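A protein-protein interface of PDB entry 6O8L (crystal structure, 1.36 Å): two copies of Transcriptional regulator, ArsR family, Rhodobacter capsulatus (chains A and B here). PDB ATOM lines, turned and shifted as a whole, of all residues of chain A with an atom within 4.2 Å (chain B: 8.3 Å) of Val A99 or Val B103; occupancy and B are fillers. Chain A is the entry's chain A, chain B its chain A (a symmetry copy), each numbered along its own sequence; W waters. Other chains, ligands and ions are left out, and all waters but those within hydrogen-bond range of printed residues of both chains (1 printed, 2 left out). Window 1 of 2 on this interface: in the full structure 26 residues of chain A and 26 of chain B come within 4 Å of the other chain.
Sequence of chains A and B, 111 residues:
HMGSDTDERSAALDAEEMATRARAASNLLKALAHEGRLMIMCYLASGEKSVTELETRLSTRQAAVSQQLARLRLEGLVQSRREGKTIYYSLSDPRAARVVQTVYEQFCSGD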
ATOM      1  N   ALA A  25     -21.080 -20.393 -14.506  1.00  0.00           N
ATOM      2  CA  ALA A  25     -20.827 -21.756 -14.954  1.00  0.00           C
ATOM      3  C   ALA A  25     -22.121 -22.559 -15.019  1.00  0.00           C
ATOM      4  O   ALA A  25     -22.333 -23.328 -15.963  1.00  0.00           O
ATOM      5  CB  ALA A  25     -19.821 -22.422 -14.018  1.00  0.00           C
ATOM      6  N   LEU A  29     -23.792 -24.729 -18.095  1.00  0.00           N
ATOM      7  CA  LEU A  29     -24.151 -26.132 -17.997  1.00  0.00           C
ATOM      8  C   LEU A  29     -25.624 -26.349 -18.310  1.00  0.00           C
ATOM      9  O   LEU A  29     -25.976 -27.371 -18.898  1.00  0.00           O
ATOM     10  CB  LEU A  29     -23.730 -26.680 -16.635  1.00  0.00           C
ATOM     11  CG  LEU A  29     -22.219 -26.613 -16.355  1.00  0.00           C
ATOM     12  CD1 LEU A  29     -21.950 -27.186 -14.977  1.00  0.00           C
ATOM     13  CD2 LEU A  29     -21.418 -27.344 -17.394  1.00  0.00           C
ATOM     14  N   LEU A  32     -25.832 -26.608 -21.913  1.00  0.00           N
ATOM     15  CA  LEU A  32     -25.284 -27.871 -22.396  1.00  0.00           C
ATOM     16  C   LEU A  32     -26.083 -29.091 -21.953  1.00  0.00           C
ATOM     17  O   LEU A  32     -25.921 -30.164 -22.551  1.00  0.00           O
ATOM     18  CB  LEU A  32     -23.840 -28.048 -21.933  1.00  0.00           C
ATOM     19  CG  LEU A  32     -22.868 -26.960 -22.373  1.00  0.00           C
ATOM     20  CD1 LEU A  32     -21.500 -27.215 -21.774  1.00  0.00           C
ATOM     21  CD2 LEU A  32     -22.787 -26.901 -23.896  1.00  0.00           C
ATOM     22  N   ARG A  95     -14.339 -21.235 -23.024  1.00  0.00           N
ATOM     23  CA  ARG A  95     -14.657 -21.978 -21.809  1.00  0.00           C
ATOM     24  C   ARG A  95     -15.555 -23.154 -22.139  1.00  0.00           C
ATOM     25  O   ARG A  95     -15.302 -24.290 -21.726  1.00  0.00           O
ATOM     26  CB  ARG A  95     -15.348 -21.070 -20.797  1.00  0.00           C
ATOM     27  CG  ARG A  95     -14.531 -19.892 -20.348  1.00  0.00           C
ATOM     28  CD  ARG A  95     -15.360 -18.919 -19.523  1.00  0.00           C
ATOM     29  NE  ARG A  95     -16.450 -18.350 -20.313  1.00  0.00           N
ATOM     30  CZ  ARG A  95     -17.278 -17.407 -19.881  1.00  0.00           C
ATOM     31  NH1 ARG A  95     -17.141 -16.921 -18.655  1.00  0.00           N
ATOM     32  NH2 ARG A  95     -18.243 -16.951 -20.676  1.00  0.00           N
ATOM     33  N   ALA A  96     -16.607 -22.897 -22.908  1.00  0.00           N
ATOM     34  CA  ALA A  96     -17.519 -23.969 -23.270  1.00  0.00           C
ATOM     35  C   ALA A  96     -16.830 -24.982 -24.158  1.00  0.00           C
ATOM     36  O   ALA A  96     -17.096 -26.186 -24.059  1.00  0.00           O
ATOM     37  CB  ALA A  96     -18.758 -23.392 -23.948  1.00  0.00           C
ATOM     38  N   ALA A  97     -15.930 -24.522 -25.028  1.00  0.00           N
ATOM     39  CA  ALA A  97     -15.233 -25.458 -25.899  1.00  0.00           C
ATOM     40  C   ALA A  97     -14.484 -26.493 -25.074  1.00  0.00           C
ATOM     41  O   ALA A  97     -14.581 -27.697 -25.331  1.00  0.00           O
ATOM     42  CB  ALA A  97     -14.292 -24.715 -26.848  1.00  0.00           C
ATOM     43  N   ARG A  98     -13.738 -26.053 -24.062  1.00  0.00           N
ATOM     44  CA  ARG A  98     -12.980 -27.021 -23.281  1.00  0.00           C
ATOM     45  C   ARG A  98     -13.901 -27.889 -22.439  1.00  0.00           C
ATOM     46  O   ARG A  98     -13.640 -29.084 -22.263  1.00  0.00           O
ATOM     47  CB  ARG A  98     -11.956 -26.325 -22.385  1.00  0.00           C
ATOM     48  CG  ARG A  98     -10.797 -25.656 -23.111  1.00  0.00           C
ATOM     49  CD  ARG A  98      -9.955 -26.643 -23.922  1.00  0.00           C
ATOM     50  NE  ARG A  98      -9.215 -27.616 -23.111  1.00  0.00           N
ATOM     51  CZ  ARG A  98      -8.057 -27.374 -22.492  1.00  0.00           C
ATOM     52  NH1 ARG A  98      -7.484 -26.175 -22.553  1.00  0.00           N
ATOM     53  NH2 ARG A  98      -7.465 -28.339 -21.796  1.00  0.00           N
ATOM     54  N   VAL A  99     -14.978 -27.311 -21.902  1.00  0.00           N
ATOM     55  CA  VAL A  99     -15.920 -28.118 -21.134  1.00  0.00           C
ATOM     56  C   VAL A  99     -16.489 -29.227 -22.008  1.00  0.00           C
ATOM     57  O   VAL A  99     -16.529 -30.401 -21.615  1.00  0.00           O
ATOM     58  CB  VAL A  99     -17.025 -27.236 -20.530  1.00  0.00           C
ATOM     59  CG1 VAL A  99     -18.127 -28.108 -19.952  1.00  0.00           C
ATOM     60  CG2 VAL A  99     -16.458 -26.317 -19.453  1.00  0.00           C
ATOM     61  N   VAL A 100     -16.937 -28.870 -23.209  1.00  0.00           N
ATOM     62  CA  VAL A 100     -17.542 -29.856 -24.093  1.00  0.00           C
ATOM     63  C   VAL A 100     -16.510 -30.878 -24.545  1.00  0.00           C
ATOM     64  O   VAL A 100     -16.808 -32.075 -24.639  1.00  0.00           O
ATOM     65  CB  VAL A 100     -18.211 -29.152 -25.283  1.00  0.00           C
ATOM     66  CG1 VAL A 100     -18.565 -30.180 -26.354  1.00  0.00           C
ATOM     67  CG2 VAL A 100     -19.416 -28.344 -24.806  1.00  0.00           C
ATOM     68  N   GLN A 101     -15.290 -30.434 -24.854  1.00  0.00           N
ATOM     69  CA  GLN A 101     -14.257 -31.398 -25.233  1.00  0.00           C
ATOM     70  C   GLN A 101     -14.009 -32.401 -24.118  1.00  0.00           C
ATOM     71  O   GLN A 101     -13.784 -33.586 -24.378  1.00  0.00           O
ATOM     72  CB  GLN A 101     -12.968 -30.677 -25.620  1.00  0.00           C
ATOM     73  CG  GLN A 101     -13.105 -30.067 -27.004  1.00  0.00           C
ATOM     74  CD  GLN A 101     -12.121 -28.984 -27.295  1.00  0.00           C
ATOM     75  OE1 GLN A 101     -11.393 -28.537 -26.416  1.00  0.00           O
ATOM     76  NE2 GLN A 101     -12.087 -28.544 -28.545  1.00  0.00           N
ATOM     77  N   THR A 102     -14.016 -31.939 -22.865  1.00  0.00           N
ATOM     78  CA  THR A 102     -13.836 -32.854 -21.745  1.00  0.00           C
ATOM     79  C   THR A 102     -15.013 -33.812 -21.649  1.00  0.00           C
ATOM     80  O   THR A 102     -14.829 -35.027 -21.503  1.00  0.00           O
ATOM     81  CB  THR A 102     -13.688 -32.057 -20.447  1.00  0.00           C
ATOM     82  OG1 THR A 102     -12.520 -31.234 -20.523  1.00  0.00           O
ATOM     83  CG2 THR A 102     -13.542 -32.958 -19.251  1.00  0.00           C
ATOM     84  N   VAL A 103     -16.233 -33.280 -21.748  1.00  0.00           N
ATOM     85  CA  VAL A 103     -17.422 -34.126 -21.740  1.00  0.00           C
ATOM     86  C   VAL A 103     -17.328 -35.192 -22.824  1.00  0.00           C
ATOM     87  O   VAL A 103     -17.543 -36.382 -22.568  1.00  0.00           O
ATOM     88  CB  VAL A 103     -18.690 -33.271 -21.901  1.00  0.00           C
ATOM     89  CG1 VAL A 103     -19.894 -34.159 -22.150  1.00  0.00           C
ATOM     90  CG2 VAL A 103     -18.893 -32.443 -20.667  1.00  0.00           C
ATOM     91  N   LEU B  29     -24.647 -33.400 -16.763  1.00  0.00           N
ATOM     92  CA  LEU B  29     -24.680 -31.949 -16.802  1.00  0.00           C
ATOM     93  C   LEU B  29     -25.910 -31.405 -16.091  1.00  0.00           C
ATOM     94  O   LEU B  29     -25.830 -30.350 -15.463  1.00  0.00           O
ATOM     95  CB  LEU B  29     -24.549 -31.468 -18.246  1.00  0.00           C
ATOM     96  CG  LEU B  29     -23.239 -31.877 -18.942  1.00  0.00           C
ATOM     97  CD1 LEU B  29     -23.246 -31.336 -20.359  1.00  0.00           C
ATOM     98  CD2 LEU B  29     -22.028 -31.391 -18.200  1.00  0.00           C
ATOM     99  N   LEU B  32     -25.018 -31.229 -12.589  1.00  0.00           N
ATOM    100  CA  LEU B  32     -24.075 -30.147 -12.326  1.00  0.00           C
ATOM    101  C   LEU B  32     -24.659 -28.759 -12.565  1.00  0.00           C
ATOM    102  O   LEU B  32     -24.086 -27.775 -12.075  1.00  0.00           O
ATOM    103  CB  LEU B  32     -22.824 -30.296 -13.186  1.00  0.00           C
ATOM    104  CG  LEU B  32     -22.048 -31.595 -13.005  1.00  0.00           C
ATOM    105  CD1 LEU B  32     -20.887 -31.647 -13.976  1.00  0.00           C
ATOM    106  CD2 LEU B  32     -21.553 -31.725 -11.566  1.00  0.00           C
ATOM    107  N   LEU B  38     -23.085 -27.496  -7.981  1.00  0.00           N
ATOM    108  CA  LEU B  38     -21.833 -27.224  -8.672  1.00  0.00           C
ATOM    109  C   LEU B  38     -20.772 -26.717  -7.705  1.00  0.00           C
ATOM    110  O   LEU B  38     -19.601 -27.101  -7.800  1.00  0.00           O
ATOM    111  CB  LEU B  38     -22.064 -26.222  -9.799  1.00  0.00           C
ATOM    112  CG  LEU B  38     -20.828 -25.838 -10.615  1.00  0.00           C
ATOM    113  CD1 LEU B  38     -20.197 -27.079 -11.234  1.00  0.00           C
ATOM    114  CD2 LEU B  38     -21.192 -24.803 -11.667  1.00  0.00           C
ATOM    115  N   CYS B  42     -17.171 -28.260  -7.104  1.00  0.00           N
ATOM    116  CA  CYS B  42     -15.947 -27.485  -7.290  1.00  0.00           C
ATOM    117  C   CYS B  42     -15.054 -27.563  -6.063  1.00  0.00           C
ATOM    118  O   CYS B  42     -13.829 -27.631  -6.191  1.00  0.00           O
ATOM    119  CB  CYS B  42     -16.248 -26.026  -7.628  1.00  0.00           C
ATOM    120  SG  CYS B  42     -16.886 -25.782  -9.297  1.00  0.00           S
ATOM    121  N   ALA B  45     -13.457 -30.885  -6.122  1.00  0.00           N
ATOM    122  CA  ALA B  45     -12.512 -31.020  -7.215  1.00  0.00           C
ATOM    123  C   ALA B  45     -11.078 -30.794  -6.774  1.00  0.00           C
ATOM    124  O   ALA B  45     -10.153 -31.194  -7.491  1.00  0.00           O
ATOM    125  CB  ALA B  45     -12.877 -30.020  -8.309  1.00  0.00           C
ATOM    126  N   ARG B  95     -15.274 -39.176 -14.610  1.00  0.00           N
ATOM    127  CA  ARG B  95     -15.741 -38.338 -15.710  1.00  0.00           C
ATOM    128  C   ARG B  95     -16.207 -36.997 -15.178  1.00  0.00           C
ATOM    129  O   ARG B  95     -15.823 -35.938 -15.685  1.00  0.00           O
ATOM    130  CB  ARG B  95     -16.883 -39.023 -16.451  1.00  0.00           C
ATOM    131  CG  ARG B  95     -16.528 -40.345 -17.072  1.00  0.00           C
ATOM    132  CD  ARG B  95     -17.761 -41.066 -17.594  1.00  0.00           C
ATOM    133  NE  ARG B  95     -18.682 -41.392 -16.507  1.00  0.00           N
ATOM    134  CZ  ARG B  95     -19.796 -42.100 -16.652  1.00  0.00           C
ATOM    135  NH1 ARG B  95     -20.131 -42.562 -17.850  1.00  0.00           N
ATOM    136  NH2 ARG B  95     -20.574 -42.344 -15.600  1.00  0.00           N
ATOM    137  N   ALA B  96     -17.026 -37.027 -14.133  1.00  0.00           N
ATOM    138  CA  ALA B  96     -17.521 -35.785 -13.564  1.00  0.00           C
ATOM    139  C   ALA B  96     -16.389 -34.992 -12.944  1.00  0.00           C
ATOM    140  O   ALA B  96     -16.384 -33.757 -13.005  1.00  0.00           O
ATOM    141  CB  ALA B  96     -18.614 -36.079 -12.542  1.00  0.00           C
ATOM    142  N   ALA B  97     -15.414 -35.680 -12.351  1.00  0.00           N
ATOM    143  CA  ALA B  97     -14.298 -34.963 -11.748  1.00  0.00           C
ATOM    144  C   ALA B  97     -13.595 -34.104 -12.786  1.00  0.00           C
ATOM    145  O   ALA B  97     -13.330 -32.920 -12.554  1.00  0.00           O
ATOM    146  CB  ALA B  97     -13.328 -35.938 -11.080  1.00  0.00           C
ATOM    147  N   ARG B  98     -13.292 -34.672 -13.953  1.00  0.00           N
ATOM    148  CA  ARG B  98     -12.583 -33.882 -14.951  1.00  0.00           C
ATOM    149  C   ARG B  98     -13.476 -32.793 -15.525  1.00  0.00           C
ATOM    150  O   ARG B  98     -13.004 -31.687 -15.809  1.00  0.00           O
ATOM    151  CB  ARG B  98     -12.049 -34.766 -16.076  1.00  0.00           C
ATOM    152  CG  ARG B  98     -10.921 -35.713 -15.687  1.00  0.00           C
ATOM    153  CD  ARG B  98      -9.677 -34.978 -15.184  1.00  0.00           C
ATOM    154  NE  ARG B  98      -8.992 -34.179 -16.205  1.00  0.00           N
ATOM    155  CZ  ARG B  98      -8.148 -34.663 -17.120  1.00  0.00           C
ATOM    156  NH1 ARG B  98      -7.879 -35.964 -17.182  1.00  0.00           N
ATOM    157  NH2 ARG B  98      -7.570 -33.840 -17.988  1.00  0.00           N
ATOM    158  N   VAL B  99     -14.765 -33.085 -15.713  1.00  0.00           N
ATOM    159  CA  VAL B  99     -15.670 -32.053 -16.209  1.00  0.00           C
ATOM    160  C   VAL B  99     -15.691 -30.873 -15.248  1.00  0.00           C
ATOM    161  O   VAL B  99     -15.566 -29.710 -15.653  1.00  0.00           O
ATOM    162  CB  VAL B  99     -17.076 -32.632 -16.442  1.00  0.00           C
ATOM    163  CG1 VAL B  99     -18.062 -31.505 -16.712  1.00  0.00           C
ATOM    164  CG2 VAL B  99     -17.071 -33.620 -17.604  1.00  0.00           C
ATOM    165  N   VAL B 100     -15.851 -31.156 -13.957  1.00  0.00           N
ATOM    166  CA  VAL B 100     -15.930 -30.088 -12.972  1.00  0.00           C
ATOM    167  C   VAL B 100     -14.602 -29.352 -12.868  1.00  0.00           C
ATOM    168  O   VAL B 100     -14.573 -28.122 -12.734  1.00  0.00           O
ATOM    169  CB  VAL B 100     -16.378 -30.655 -11.617  1.00  0.00           C
ATOM    170  CG1 VAL B 100     -16.162 -29.612 -10.526  1.00  0.00           C
ATOM    171  CG2 VAL B 100     -17.823 -31.143 -11.703  1.00  0.00           C
ATOM    172  N   GLN B 101     -13.484 -30.080 -12.903  1.00  0.00           N
ATOM    173  CA  GLN B 101     -12.192 -29.397 -12.868  1.00  0.00           C
ATOM    174  C   GLN B 101     -12.043 -28.443 -14.042  1.00  0.00           C
ATOM    175  O   GLN B 101     -11.482 -27.353 -13.897  1.00  0.00           O
ATOM    176  CB  GLN B 101     -11.051 -30.413 -12.839  1.00  0.00           C
ATOM    177  CG  GLN B 101     -10.927 -31.022 -11.453  1.00  0.00           C
ATOM    178  CD  GLN B 101     -10.184 -32.314 -11.417  1.00  0.00           C
ATOM    179  OE1 GLN B 101      -9.861 -32.889 -12.451  1.00  0.00           O
ATOM    180  NE2 GLN B 101      -9.898 -32.793 -10.214  1.00  0.00           N
ATOM    181  N   THR B 102     -12.514 -28.846 -15.223  1.00  0.00           N
ATOM    182  CA  THR B 102     -12.452 -27.961 -16.380  1.00  0.00           C
ATOM    183  C   THR B 102     -13.348 -26.751 -16.169  1.00  0.00           C
ATOM    184  O   THR B 102     -12.935 -25.609 -16.404  1.00  0.00           O
ATOM    185  CB  THR B 102     -12.869 -28.725 -17.638  1.00  0.00           C
ATOM    186  OG1 THR B 102     -11.955 -29.801 -17.869  1.00  0.00           O
ATOM    187  CG2 THR B 102     -12.864 -27.842 -18.856  1.00  0.00           C
ATOM    188  N   VAL B 103     -14.579 -26.987 -15.709  1.00  0.00           N
ATOM    189  CA  VAL B 103     -15.489 -25.886 -15.407  1.00  0.00           C
ATOM    190  C   VAL B 103     -14.844 -24.909 -14.432  1.00  0.00           C
ATOM    191  O   VAL B 103     -14.838 -23.693 -14.658  1.00  0.00           O
ATOM    192  CB  VAL B 103     -16.822 -26.425 -14.863  1.00  0.00           C
ATOM    193  CG1 VAL B 103     -17.663 -25.289 -14.313  1.00  0.00           C
ATOM    194  CG2 VAL B 103     -17.555 -27.139 -15.959  1.00  0.00           C
ATOM    195  N   TYR B 104     -14.312 -25.432 -13.320  1.00  0.00           N
ATOM    196  CA  TYR B 104     -13.727 -24.609 -12.261  1.00  0.00           C
ATOM    197  C   TYR B 104     -12.583 -23.772 -12.805  1.00  0.00           C
ATOM    198  O   TYR B 104     -12.512 -22.559 -12.579  1.00  0.00           O
ATOM    199  CB  TYR B 104     -13.225 -25.565 -11.167  1.00  0.00           C
ATOM    200  CG  TYR B 104     -12.696 -25.007  -9.852  1.00  0.00           C
ATOM    201  CD1 TYR B 104     -13.329 -23.980  -9.213  1.00  0.00           C
ATOM    202  CD2 TYR B 104     -11.575 -25.575  -9.228  1.00  0.00           C
ATOM    203  CE1 TYR B 104     -12.856 -23.500  -7.992  1.00  0.00           C
ATOM    204  CE2 TYR B 104     -11.094 -25.103  -8.014  1.00  0.00           C
ATOM    205  CZ  TYR B 104     -11.742 -24.082  -7.394  1.00  0.00           C
ATOM    206  OH  TYR B 104     -11.227 -23.655  -6.186  1.00  0.00           O
ATOM    207  N   GLU B 105     -11.679 -24.406 -13.537  1.00  0.00           N
ATOM    208  CA  GLU B 105     -10.537 -23.680 -14.058  1.00  0.00           C
ATOM    209  C   GLU B 105     -10.966 -22.640 -15.080  1.00  0.00           C
ATOM    210  O   GLU B 105     -10.500 -21.496 -15.047  1.00  0.00           O
ATOM    211  CB  GLU B 105      -9.560 -24.672 -14.660  1.00  0.00           C
ATOM    212  CG  GLU B 105      -8.408 -24.047 -15.380  1.00  0.00           C
ATOM    213  CD  GLU B 105      -7.423 -25.080 -15.816  1.00  0.00           C
ATOM    214  OE1 GLU B 105      -6.562 -25.450 -14.990  1.00  0.00           O
ATOM    215  OE2 GLU B 105      -7.512 -25.527 -16.983  1.00  0.00           O
ATOM    216  N   GLN B 106     -11.858 -23.018 -15.994  1.00  0.00           N
ATOM    217  CA  GLN B 106     -12.242 -22.105 -17.061  1.00  0.00           C
ATOM    218  C   GLN B 106     -12.953 -20.880 -16.506  1.00  0.00           C
ATOM    219  O   GLN B 106     -12.682 -19.753 -16.933  1.00  0.00           O
ATOM    220  CB  GLN B 106     -13.123 -22.831 -18.079  1.00  0.00           C
ATOM    221  CG  GLN B 106     -12.358 -23.831 -18.938  1.00  0.00           C
ATOM    222  CD  GLN B 106     -11.326 -23.169 -19.837  1.00  0.00           C
ATOM    223  OE1 GLN B 106     -11.512 -22.050 -20.325  1.00  0.00           O
ATOM    224  NE2 GLN B 106     -10.245 -23.885 -20.088  1.00  0.00           N
ATOM    225  N   PHE B 107     -13.874 -21.080 -15.564  1.00  0.00           N
ATOM    226  CA  PHE B 107     -14.670 -19.975 -15.053  1.00  0.00           C
ATOM    227  C   PHE B 107     -13.952 -19.147 -13.999  1.00  0.00           C
ATOM    228  O   PHE B 107     -14.394 -18.028 -13.715  1.00  0.00           O
ATOM    229  CB  PHE B 107     -16.043 -20.475 -14.603  1.00  0.00           C
ATOM    230  CG  PHE B 107     -16.980 -20.648 -15.748  1.00  0.00           C
ATOM    231  CD1 PHE B 107     -17.832 -19.621 -16.119  1.00  0.00           C
ATOM    232  CD2 PHE B 107     -16.955 -21.805 -16.510  1.00  0.00           C
ATOM    233  CE1 PHE B 107     -18.658 -19.753 -17.197  1.00  0.00           C
ATOM    234  CE2 PHE B 107     -17.796 -21.943 -17.599  1.00  0.00           C
ATOM    235  CZ  PHE B 107     -18.644 -20.913 -17.938  1.00  0.00           C
ATOM    236  N   CYS B 108     -12.844 -19.639 -13.447  1.00  0.00           N
ATOM    237  CA  CYS B 108     -11.998 -18.841 -12.570  1.00  0.00           C
ATOM    238  C   CYS B 108     -10.904 -18.108 -13.322  1.00  0.00           C
ATOM    239  O   CYS B 108     -10.152 -17.346 -12.704  1.00  0.00           O
ATOM    240  CB  CYS B 108     -11.325 -19.721 -11.524  1.00  0.00           C
ATOM    241  SG  CYS B 108     -12.455 -20.311 -10.286  1.00  0.00           S
ATOM    242  N   SER B 109     -10.787 -18.319 -14.628  1.00  0.00           N
ATOM    243  CA  SER B 109      -9.745 -17.699 -15.437  1.00  0.00           C
ATOM    244  C   SER B 109     -10.349 -16.592 -16.282  1.00  0.00           C
ATOM    245  O   SER B 109     -11.013 -16.873 -17.290  1.00  0.00           O
ATOM    246  CB  SER B 109      -9.116 -18.734 -16.361  1.00  0.00           C
ATOM    247  OG  SER B 109      -8.576 -19.814 -15.617  1.00  0.00           O
HETATM  248  O   HOH W   1      -8.619 -23.553 -22.791  1.00  0.00           O
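O of Arg A98 lies within hydrogen-bond range of OG1 of Thr A102 (3.0 Å).
O of Leu B38 is in hydrogen-bond range of SG of Cys B42.
The backbone carbonyl oxygen (O) of Arg B98 lies within hydrogen-bond range of the side-chain hydroxyl (OG1) of Thr B102, 3.0 Å away.
Water W1 lies within hydrogen-bond range of NH1 of Arg A98 (2.9 Å) and NE2 of Gln B106 (3.2 Å).
Arg A98 touches Thr B102, and with the chains exchanged Thr A102 touches Arg B98.
Val A99 touches Thr B102, and with the chains exchanged Thr A102 touches Val B99.
Val A99 touches Val B103, and with the chains exchanged Val A103 touches Val B99.
Thr A102 touches its own counterpart, Thr B102.
11 positions are printed for both chains.
Of the 15 pairs that touch across the chains among the printed residues, 9 have their exchanged pair printed and touching as well.
Printed residues of chain B that touch a printed residue of chain A: Leu B29, Leu B32, Leu B38, Arg B98, Val B99, Thr B102, Val B103, Gln B106 and Phe B107.
Among the printed residues, no Asp or Glu carboxylate lies within 4 Å of a Lys or Arg side-chain nitrogen of the other chain.
Among the printed residues, merely in contact across the chains: Ala A25 with Leu B38 (3.6 Å), Ala A25 with Val B103 (3.6 Å), Ala A25 with Phe B107 (3.7 Å), Leu A29 with Leu B32 (3.7 Å), Leu A32 with Leu B29 (3.7 Å), Arg A95 with Gln B106 (3.5 Å), Arg A95 with Phe B107 (3.5 Å), Arg A98 with Thr B102 (3.7 Å), Arg A98 with Gln B106 (3.5 Å), Val A99 with Thr B102 (3.7 Å), Val A99 with Val B103 (3.8 Å), Thr A102 with Arg B98 (3.7 Å), Thr A102 with Val B99 (3.7 Å) and Val A103 with Val B99 (3.8 Å).
Val A99 touches just these residues of chain B: Thr B102 and Val B103.
Val B103 touches just these residues of chain A: Ala A25 (3.6 Å) and Val A99 (3.8 Å).
Of the printed residues of chain A, Arg B98 touches Thr A102 (3.7 Å).
Of the printed residues of chain A, Val B99 touches Thr A102 and Val A103.
Of the printed residues of chain B, Leu A29 touches Leu B32 (3.7 Å).
Cys B42 touches none of the printed residues of chain A.
The nearest residue of chain A that does not touch Val B103 is Leu A29 (4.1 Å).
The nearest printed residue of chain B that does not touch Leu A32 is Val B103 (7.0 Å).
The side-chain hydroxyl of Thr B102 lies within hydrogen-bond range of the side-chain hydroxyl of Thr A102 (3.1 Å).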
